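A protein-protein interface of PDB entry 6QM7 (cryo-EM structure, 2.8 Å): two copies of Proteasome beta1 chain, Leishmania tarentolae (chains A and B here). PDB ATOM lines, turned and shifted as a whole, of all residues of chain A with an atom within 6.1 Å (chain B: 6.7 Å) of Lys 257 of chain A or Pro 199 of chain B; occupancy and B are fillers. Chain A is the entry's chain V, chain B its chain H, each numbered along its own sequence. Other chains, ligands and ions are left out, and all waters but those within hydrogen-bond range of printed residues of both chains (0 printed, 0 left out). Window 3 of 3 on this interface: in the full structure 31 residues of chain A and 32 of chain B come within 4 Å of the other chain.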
ATOM      1  N   TYR A 250     -22.119 -17.448 -25.455  1.00  0.00           N
ATOM      2  CA  TYR A 250     -21.666 -16.625 -24.315  1.00  0.00           C
ATOM      3  C   TYR A 250     -21.609 -15.159 -24.726  1.00  0.00           C
ATOM      4  O   TYR A 250     -21.210 -14.858 -25.856  1.00  0.00           O
ATOM      5  CB  TYR A 250     -20.286 -17.064 -23.816  1.00  0.00           C
ATOM      6  CG  TYR A 250     -19.829 -16.273 -22.620  1.00  0.00           C
ATOM      7  CD1 TYR A 250     -19.006 -15.172 -22.767  1.00  0.00           C
ATOM      8  CD2 TYR A 250     -20.281 -16.577 -21.350  1.00  0.00           C
ATOM      9  CE1 TYR A 250     -18.602 -14.418 -21.676  1.00  0.00           C
ATOM     10  CE2 TYR A 250     -19.890 -15.833 -20.251  1.00  0.00           C
ATOM     11  CZ  TYR A 250     -19.054 -14.745 -20.412  1.00  0.00           C
ATOM     12  OH  TYR A 250     -18.680 -14.000 -19.334  1.00  0.00           O
ATOM     13  N   ASP A 255     -24.308 -12.970 -18.889  1.00  0.00           N
ATOM     14  CA  ASP A 255     -23.640 -13.804 -17.852  1.00  0.00           C
ATOM     15  C   ASP A 255     -24.032 -13.265 -16.483  1.00  0.00           C
ATOM     16  O   ASP A 255     -23.727 -12.109 -16.201  1.00  0.00           O
ATOM     17  CB  ASP A 255     -22.117 -13.759 -18.016  1.00  0.00           C
ATOM     18  CG  ASP A 255     -21.315 -14.700 -17.129  1.00  0.00           C
ATOM     19  OD1 ASP A 255     -20.075 -14.689 -17.242  1.00  0.00           O
ATOM     20  OD2 ASP A 255     -21.928 -15.443 -16.341  1.00  0.00           O
ATOM     21  N   PRO A 256     -24.724 -14.040 -15.611  1.00  0.00           N
ATOM     22  CA  PRO A 256     -25.208 -13.513 -14.322  1.00  0.00           C
ATOM     23  C   PRO A 256     -24.120 -13.007 -13.353  1.00  0.00           C
ATOM     24  O   PRO A 256     -24.411 -12.156 -12.533  1.00  0.00           O
ATOM     25  CB  PRO A 256     -25.977 -14.697 -13.710  1.00  0.00           C
ATOM     26  CG  PRO A 256     -25.449 -15.914 -14.438  1.00  0.00           C
ATOM     27  CD  PRO A 256     -25.128 -15.438 -15.836  1.00  0.00           C
ATOM     28  N   LYS A 257     -22.910 -13.557 -13.474  1.00  0.00           N
ATOM     29  CA  LYS A 257     -21.635 -13.094 -12.855  1.00  0.00           C
ATOM     30  C   LYS A 257     -21.490 -11.572 -12.883  1.00  0.00           C
ATOM     31  O   LYS A 257     -20.892 -11.049 -11.947  1.00  0.00           O
ATOM     32  CB  LYS A 257     -20.445 -13.626 -13.661  1.00  0.00           C
ATOM     33  CG  LYS A 257     -19.453 -14.496 -12.908  1.00  0.00           C
ATOM     34  CD  LYS A 257     -18.047 -14.511 -13.499  1.00  0.00           C
ATOM     35  CE  LYS A 257     -17.954 -14.760 -14.991  1.00  0.00           C
ATOM     36  NZ  LYS A 257     -18.445 -16.105 -15.376  1.00  0.00           N
ATOM     37  N   TYR A 258     -21.921 -10.917 -13.966  1.00  0.00           N
ATOM     38  CA  TYR A 258     -21.689  -9.476 -14.257  1.00  0.00           C
ATOM     39  C   TYR A 258     -23.006  -8.688 -14.303  1.00  0.00           C
ATOM     40  O   TYR A 258     -23.068  -7.687 -15.044  1.00  0.00           O
ATOM     41  CB  TYR A 258     -20.956  -9.314 -15.590  1.00  0.00           C
ATOM     42  CG  TYR A 258     -19.650 -10.061 -15.698  1.00  0.00           C
ATOM     43  CD1 TYR A 258     -18.609  -9.805 -14.820  1.00  0.00           C
ATOM     44  CD2 TYR A 258     -19.433 -11.001 -16.697  1.00  0.00           C
ATOM     45  CE1 TYR A 258     -17.403 -10.486 -14.908  1.00  0.00           C
ATOM     46  CE2 TYR A 258     -18.226 -11.674 -16.814  1.00  0.00           C
ATOM     47  CZ  TYR A 258     -17.212 -11.420 -15.909  1.00  0.00           C
ATOM     48  OH  TYR A 258     -16.025 -12.083 -16.001  1.00  0.00           O
ATOM     49  N   VAL A 259     -24.015  -9.078 -13.522  1.00  0.00           N
ATOM     50  CA  VAL A 259     -25.303  -8.326 -13.439  1.00  0.00           C
ATOM     51  C   VAL A 259     -25.153  -7.236 -12.380  1.00  0.00           C
ATOM     52  O   VAL A 259     -25.407  -6.053 -12.703  1.00  0.00           O
ATOM     53  CB  VAL A 259     -26.491  -9.250 -13.133  1.00  0.00           C
ATOM     54  CG1 VAL A 259     -27.684  -8.497 -12.568  1.00  0.00           C
ATOM     55  CG2 VAL A 259     -26.877 -10.035 -14.379  1.00  0.00           C
ATOM     56  N   THR A 260     -24.784  -7.628 -11.159  1.00  0.00           N
ATOM     57  CA  THR A 260     -24.526  -6.695 -10.033  1.00  0.00           C
ATOM     58  C   THR A 260     -23.446  -5.714 -10.488  1.00  0.00           C
ATOM     59  O   THR A 260     -22.372  -6.175 -10.925  1.00  0.00           O
ATOM     60  CB  THR A 260     -24.153  -7.453  -8.754  1.00  0.00           C
ATOM     61  OG1 THR A 260     -25.314  -8.184  -8.350  1.00  0.00           O
ATOM     62  CG2 THR A 260     -23.701  -6.547  -7.632  1.00  0.00           C
ATOM     63  N   SER B  61     -13.034 -12.471  -4.411  1.00  0.00           N
ATOM     64  CA  SER B  61     -13.842 -12.443  -3.174  1.00  0.00           C
ATOM     65  C   SER B  61     -14.530 -13.795  -3.031  1.00  0.00           C
ATOM     66  O   SER B  61     -15.093 -14.272  -4.033  1.00  0.00           O
ATOM     67  CB  SER B  61     -14.843 -11.331  -3.221  1.00  0.00           C
ATOM     68  OG  SER B  61     -14.230 -10.079  -3.479  1.00  0.00           O
ATOM     69  N   ASP B 178     -15.730  -7.852  -7.723  1.00  0.00           N
ATOM     70  CA  ASP B 178     -15.896  -9.175  -7.074  1.00  0.00           C
ATOM     71  C   ASP B 178     -14.547  -9.886  -7.215  1.00  0.00           C
ATOM     72  O   ASP B 178     -14.109 -10.557  -6.264  1.00  0.00           O
ATOM     73  CB  ASP B 178     -17.094  -9.925  -7.669  1.00  0.00           C
ATOM     74  CG  ASP B 178     -17.161 -11.401  -7.300  1.00  0.00           C
ATOM     75  OD1 ASP B 178     -17.053 -11.716  -6.086  1.00  0.00           O
ATOM     76  OD2 ASP B 178     -17.307 -12.230  -8.231  1.00  0.00           O
ATOM     77  N   TYR B 179     -13.905  -9.712  -8.360  1.00  0.00           N
ATOM     78  CA  TYR B 179     -12.549 -10.240  -8.621  1.00  0.00           C
ATOM     79  C   TYR B 179     -11.790  -9.274  -9.522  1.00  0.00           C
ATOM     80  O   TYR B 179     -12.409  -8.587 -10.332  1.00  0.00           O
ATOM     81  CB  TYR B 179     -12.656 -11.620  -9.263  1.00  0.00           C
ATOM     82  CG  TYR B 179     -13.071 -11.624 -10.711  1.00  0.00           C
ATOM     83  CD1 TYR B 179     -12.126 -11.509 -11.707  1.00  0.00           C
ATOM     84  CD2 TYR B 179     -14.395 -11.738 -11.086  1.00  0.00           C
ATOM     85  CE1 TYR B 179     -12.473 -11.491 -13.044  1.00  0.00           C
ATOM     86  CE2 TYR B 179     -14.764 -11.746 -12.419  1.00  0.00           C
ATOM     87  CZ  TYR B 179     -13.797 -11.628 -13.401  1.00  0.00           C
ATOM     88  OH  TYR B 179     -14.140 -11.619 -14.721  1.00  0.00           O
ATOM     89  N   TYR B 190      -8.989 -13.394 -18.441  1.00  0.00           N
ATOM     90  CA  TYR B 190     -10.338 -12.789 -18.595  1.00  0.00           C
ATOM     91  C   TYR B 190     -11.313 -13.826 -19.154  1.00  0.00           C
ATOM     92  O   TYR B 190     -12.453 -13.911 -18.669  1.00  0.00           O
ATOM     93  CB  TYR B 190     -10.309 -11.547 -19.479  1.00  0.00           C
ATOM     94  CG  TYR B 190      -9.728 -10.359 -18.770  1.00  0.00           C
ATOM     95  CD1 TYR B 190     -10.380  -9.763 -17.704  1.00  0.00           C
ATOM     96  CD2 TYR B 190      -8.492  -9.868 -19.140  1.00  0.00           C
ATOM     97  CE1 TYR B 190      -9.820  -8.684 -17.041  1.00  0.00           C
ATOM     98  CE2 TYR B 190      -7.919  -8.792 -18.484  1.00  0.00           C
ATOM     99  CZ  TYR B 190      -8.584  -8.194 -17.435  1.00  0.00           C
ATOM    100  OH  TYR B 190      -7.970  -7.142 -16.812  1.00  0.00           O
ATOM    101  N   PHE B 193     -11.861 -16.772 -16.553  1.00  0.00           N
ATOM    102  CA  PHE B 193     -12.823 -16.361 -15.501  1.00  0.00           C
ATOM    103  C   PHE B 193     -14.227 -16.368 -16.092  1.00  0.00           C
ATOM    104  O   PHE B 193     -15.109 -17.025 -15.535  1.00  0.00           O
ATOM    105  CB  PHE B 193     -12.464 -14.997 -14.906  1.00  0.00           C
ATOM    106  CG  PHE B 193     -11.548 -15.102 -13.714  1.00  0.00           C
ATOM    107  CD1 PHE B 193     -12.022 -14.876 -12.434  1.00  0.00           C
ATOM    108  CD2 PHE B 193     -10.221 -15.469 -13.871  1.00  0.00           C
ATOM    109  CE1 PHE B 193     -11.183 -15.003 -11.340  1.00  0.00           C
ATOM    110  CE2 PHE B 193      -9.380 -15.588 -12.780  1.00  0.00           C
ATOM    111  CZ  PHE B 193      -9.862 -15.361 -11.515  1.00  0.00           C
ATOM    112  N   ASP B 194     -14.419 -15.690 -17.218  1.00  0.00           N
ATOM    113  CA  ASP B 194     -15.715 -15.655 -17.944  1.00  0.00           C
ATOM    114  C   ASP B 194     -16.302 -17.066 -18.031  1.00  0.00           C
ATOM    115  O   ASP B 194     -17.519 -17.203 -17.829  1.00  0.00           O
ATOM    116  CB  ASP B 194     -15.540 -15.074 -19.347  1.00  0.00           C
ATOM    117  CG  ASP B 194     -15.395 -13.564 -19.398  1.00  0.00           C
ATOM    118  OD1 ASP B 194     -15.074 -13.043 -20.495  1.00  0.00           O
ATOM    119  OD2 ASP B 194     -15.601 -12.919 -18.357  1.00  0.00           O
ATOM    120  N   ALA B 195     -15.468 -18.066 -18.313  1.00  0.00           N
ATOM    121  CA  ALA B 195     -15.902 -19.456 -18.576  1.00  0.00           C
ATOM    122  C   ALA B 195     -16.023 -20.271 -17.281  1.00  0.00           C
ATOM    123  O   ALA B 195     -17.050 -20.964 -17.127  1.00  0.00           O
ATOM    124  CB  ALA B 195     -14.951 -20.107 -19.542  1.00  0.00           C
ATOM    125  N   ASN B 196     -15.020 -20.206 -16.403  1.00  0.00           N
ATOM    126  CA  ASN B 196     -14.839 -21.181 -15.296  1.00  0.00           C
ATOM    127  C   ASN B 196     -15.147 -20.552 -13.935  1.00  0.00           C
ATOM    128  O   ASN B 196     -15.526 -21.314 -13.025  1.00  0.00           O
ATOM    129  CB  ASN B 196     -13.444 -21.807 -15.342  1.00  0.00           C
ATOM    130  CG  ASN B 196     -13.083 -22.308 -16.725  1.00  0.00           C
ATOM    131  OD1 ASN B 196     -13.906 -22.904 -17.419  1.00  0.00           O
ATOM    132  ND2 ASN B 196     -11.859 -22.046 -17.142  1.00  0.00           N
ATOM    133  N   TYR B 197     -14.993 -19.240 -13.770  1.00  0.00           N
ATOM    134  CA  TYR B 197     -15.262 -18.572 -12.472  1.00  0.00           C
ATOM    135  C   TYR B 197     -16.764 -18.543 -12.219  1.00  0.00           C
ATOM    136  O   TYR B 197     -17.534 -18.118 -13.090  1.00  0.00           O
ATOM    137  CB  TYR B 197     -14.717 -17.148 -12.396  1.00  0.00           C
ATOM    138  CG  TYR B 197     -14.943 -16.472 -11.064  1.00  0.00           C
ATOM    139  CD1 TYR B 197     -14.439 -17.008  -9.891  1.00  0.00           C
ATOM    140  CD2 TYR B 197     -15.663 -15.293 -10.973  1.00  0.00           C
ATOM    141  CE1 TYR B 197     -14.643 -16.388  -8.668  1.00  0.00           C
ATOM    142  CE2 TYR B 197     -15.874 -14.660  -9.762  1.00  0.00           C
ATOM    143  CZ  TYR B 197     -15.359 -15.205  -8.603  1.00  0.00           C
ATOM    144  OH  TYR B 197     -15.560 -14.585  -7.401  1.00  0.00           O
ATOM    145  N   LYS B 198     -17.134 -19.019 -11.038  1.00  0.00           N
ATOM    146  CA  LYS B 198     -18.498 -18.977 -10.472  1.00  0.00           C
ATOM    147  C   LYS B 198     -18.377 -18.266  -9.131  1.00  0.00           C
ATOM    148  O   LYS B 198     -17.636 -18.722  -8.266  1.00  0.00           O
ATOM    149  CB  LYS B 198     -19.003 -20.413 -10.320  1.00  0.00           C
ATOM    150  CG  LYS B 198     -20.508 -20.571 -10.422  1.00  0.00           C
ATOM    151  CD  LYS B 198     -21.014 -20.544 -11.851  1.00  0.00           C
ATOM    152  CE  LYS B 198     -22.516 -20.726 -11.940  1.00  0.00           C
ATOM    153  NZ  LYS B 198     -22.929 -21.200 -13.282  1.00  0.00           N
ATOM    154  N   PRO B 199     -19.042 -17.114  -8.902  1.00  0.00           N
ATOM    155  CA  PRO B 199     -18.977 -16.464  -7.594  1.00  0.00           C
ATOM    156  C   PRO B 199     -19.740 -17.282  -6.536  1.00  0.00           C
ATOM    157  O   PRO B 199     -20.452 -18.226  -6.896  1.00  0.00           O
ATOM    158  CB  PRO B 199     -19.592 -15.079  -7.850  1.00  0.00           C
ATOM    159  CG  PRO B 199     -20.542 -15.312  -9.013  1.00  0.00           C
ATOM    160  CD  PRO B 199     -19.885 -16.384  -9.857  1.00  0.00           C
ATOM    161  N   GLY B 200     -19.566 -16.906  -5.264  1.00  0.00           N
ATOM    162  CA  GLY B 200     -20.076 -17.645  -4.094  1.00  0.00           C
ATOM    163  C   GLY B 200     -19.342 -18.959  -3.896  1.00  0.00           C
ATOM    164  O   GLY B 200     -19.993 -19.948  -3.506  1.00  0.00           O
ATOM    165  N   MET B 201     -18.030 -18.966  -4.145  1.00  0.00           N
ATOM    166  CA  MET B 201     -17.124 -20.104  -3.836  1.00  0.00           C
ATOM    167  C   MET B 201     -16.834 -20.102  -2.331  1.00  0.00           C
ATOM    168  O   MET B 201     -16.933 -19.027  -1.702  1.00  0.00           O
ATOM    169  CB  MET B 201     -15.793 -19.995  -4.589  1.00  0.00           C
ATOM    170  CG  MET B 201     -15.786 -20.622  -5.982  1.00  0.00           C
ATOM    171  SD  MET B 201     -14.310 -20.108  -6.927  1.00  0.00           S
ATOM    172  CE  MET B 201     -14.460 -21.132  -8.391  1.00  0.00           C
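No position is printed for both chains.
Of the 8 pairs that touch across the chains among the printed residues, none has its exchanged pair printed and touching as well.
Printed residues of chain B within 4 Å of Tyr 250 of chain A: Asp 194 (3.3 Å).
Of the printed residues of chain B, Asp 255 of chain A touches Asp 194.
Lys 257 of chain A touches four residues of chain B.
Printed residues of chain B within 4 Å of Tyr 258 of chain A: Tyr 179 and Asp 194.
Val 259 of chain A touches none of the printed residues of chain B.
Asp 178 of chain B touches none of the printed residues of chain A.
Printed residues of chain A within 4 Å of Tyr 179 of chain B: Tyr 258 (2.3 Å).
Of the printed residues of chain A, Phe 193 of chain B touches Lys 257 (3.5 Å).
The nearest printed residue of chain B that does not touch Tyr 250 of chain A is Ala 195 of chain B (5.3 Å).
The side-chain hydroxyl (OH) of Tyr 179 of chain B sits close to the side-chain hydroxyl (OH) of Tyr 258 of chain A (2.3 Å).
The backbone carbonyl oxygen of Phe 193 of chain B sits at hydrogen-bond distance from the side-chain amino group of Lys 257 of chain A, at 3.5 Å.
OD2 of Asp 194 of chain B sits at hydrogen-bond distance from OH of Tyr 258 of chain A (2.5 Å).
OD2 of Asp 194 of chain B sits close to OH of Tyr 250 of chain A (3.4 Å).
The side-chain amino group of Lys 257 of chain A lies within hydrogen-bond range of the backbone carbonyl oxygen of Asp 194 of chain B, at 2.8 Å.
The side-chain amino group (NZ) of Lys 257 of chain A lies within hydrogen-bond range of the backbone carbonyl oxygen (O) of Tyr 197 of chain B (3.2 Å).
Of the 7 printed residues of chain A, 4 touch a printed residue of chain B.
Hydrophobic or aromatic side chains of chain A within 4 Å of the printed part of chain B: Tyr 250 and Tyr 258.
Hydrophobic or aromatic side chains of chain B within 4 Å of the printed part of chain A: Tyr 179, Tyr 197 and Pro 199.
Among the printed residues, no Asp or Glu carboxylate lies within 4 Å of a Lys or Arg side-chain nitrogen of the other chain.
OH of Tyr 250 of chain A is in hydrogen-bond range of OD1 of Asp 255 of chain A (2.6 Å).
The side-chain carboxylate (OD2) of Asp 178 of chain B is in hydrogen-bond range of the side-chain hydroxyl (OH) of Tyr 197 of chain B (3.0 Å).
O of Ser 61 of chain B is in hydrogen-bond range of OH of Tyr 197 of chain B (3.4 Å).
The side-chain amino group (NZ) of Lys 257 of chain A is in salt-bridge range of the side-chain carboxylate (OD1) of Asp 255 of chain A, 2.9 Å away.
OD1 of Asp 255 of chain A touches O of Asp 194 of chain B, 3.6 Å away.
CG of Lys 257 of chain A touches CD of Pro 199 of chain B (3.6 Å).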
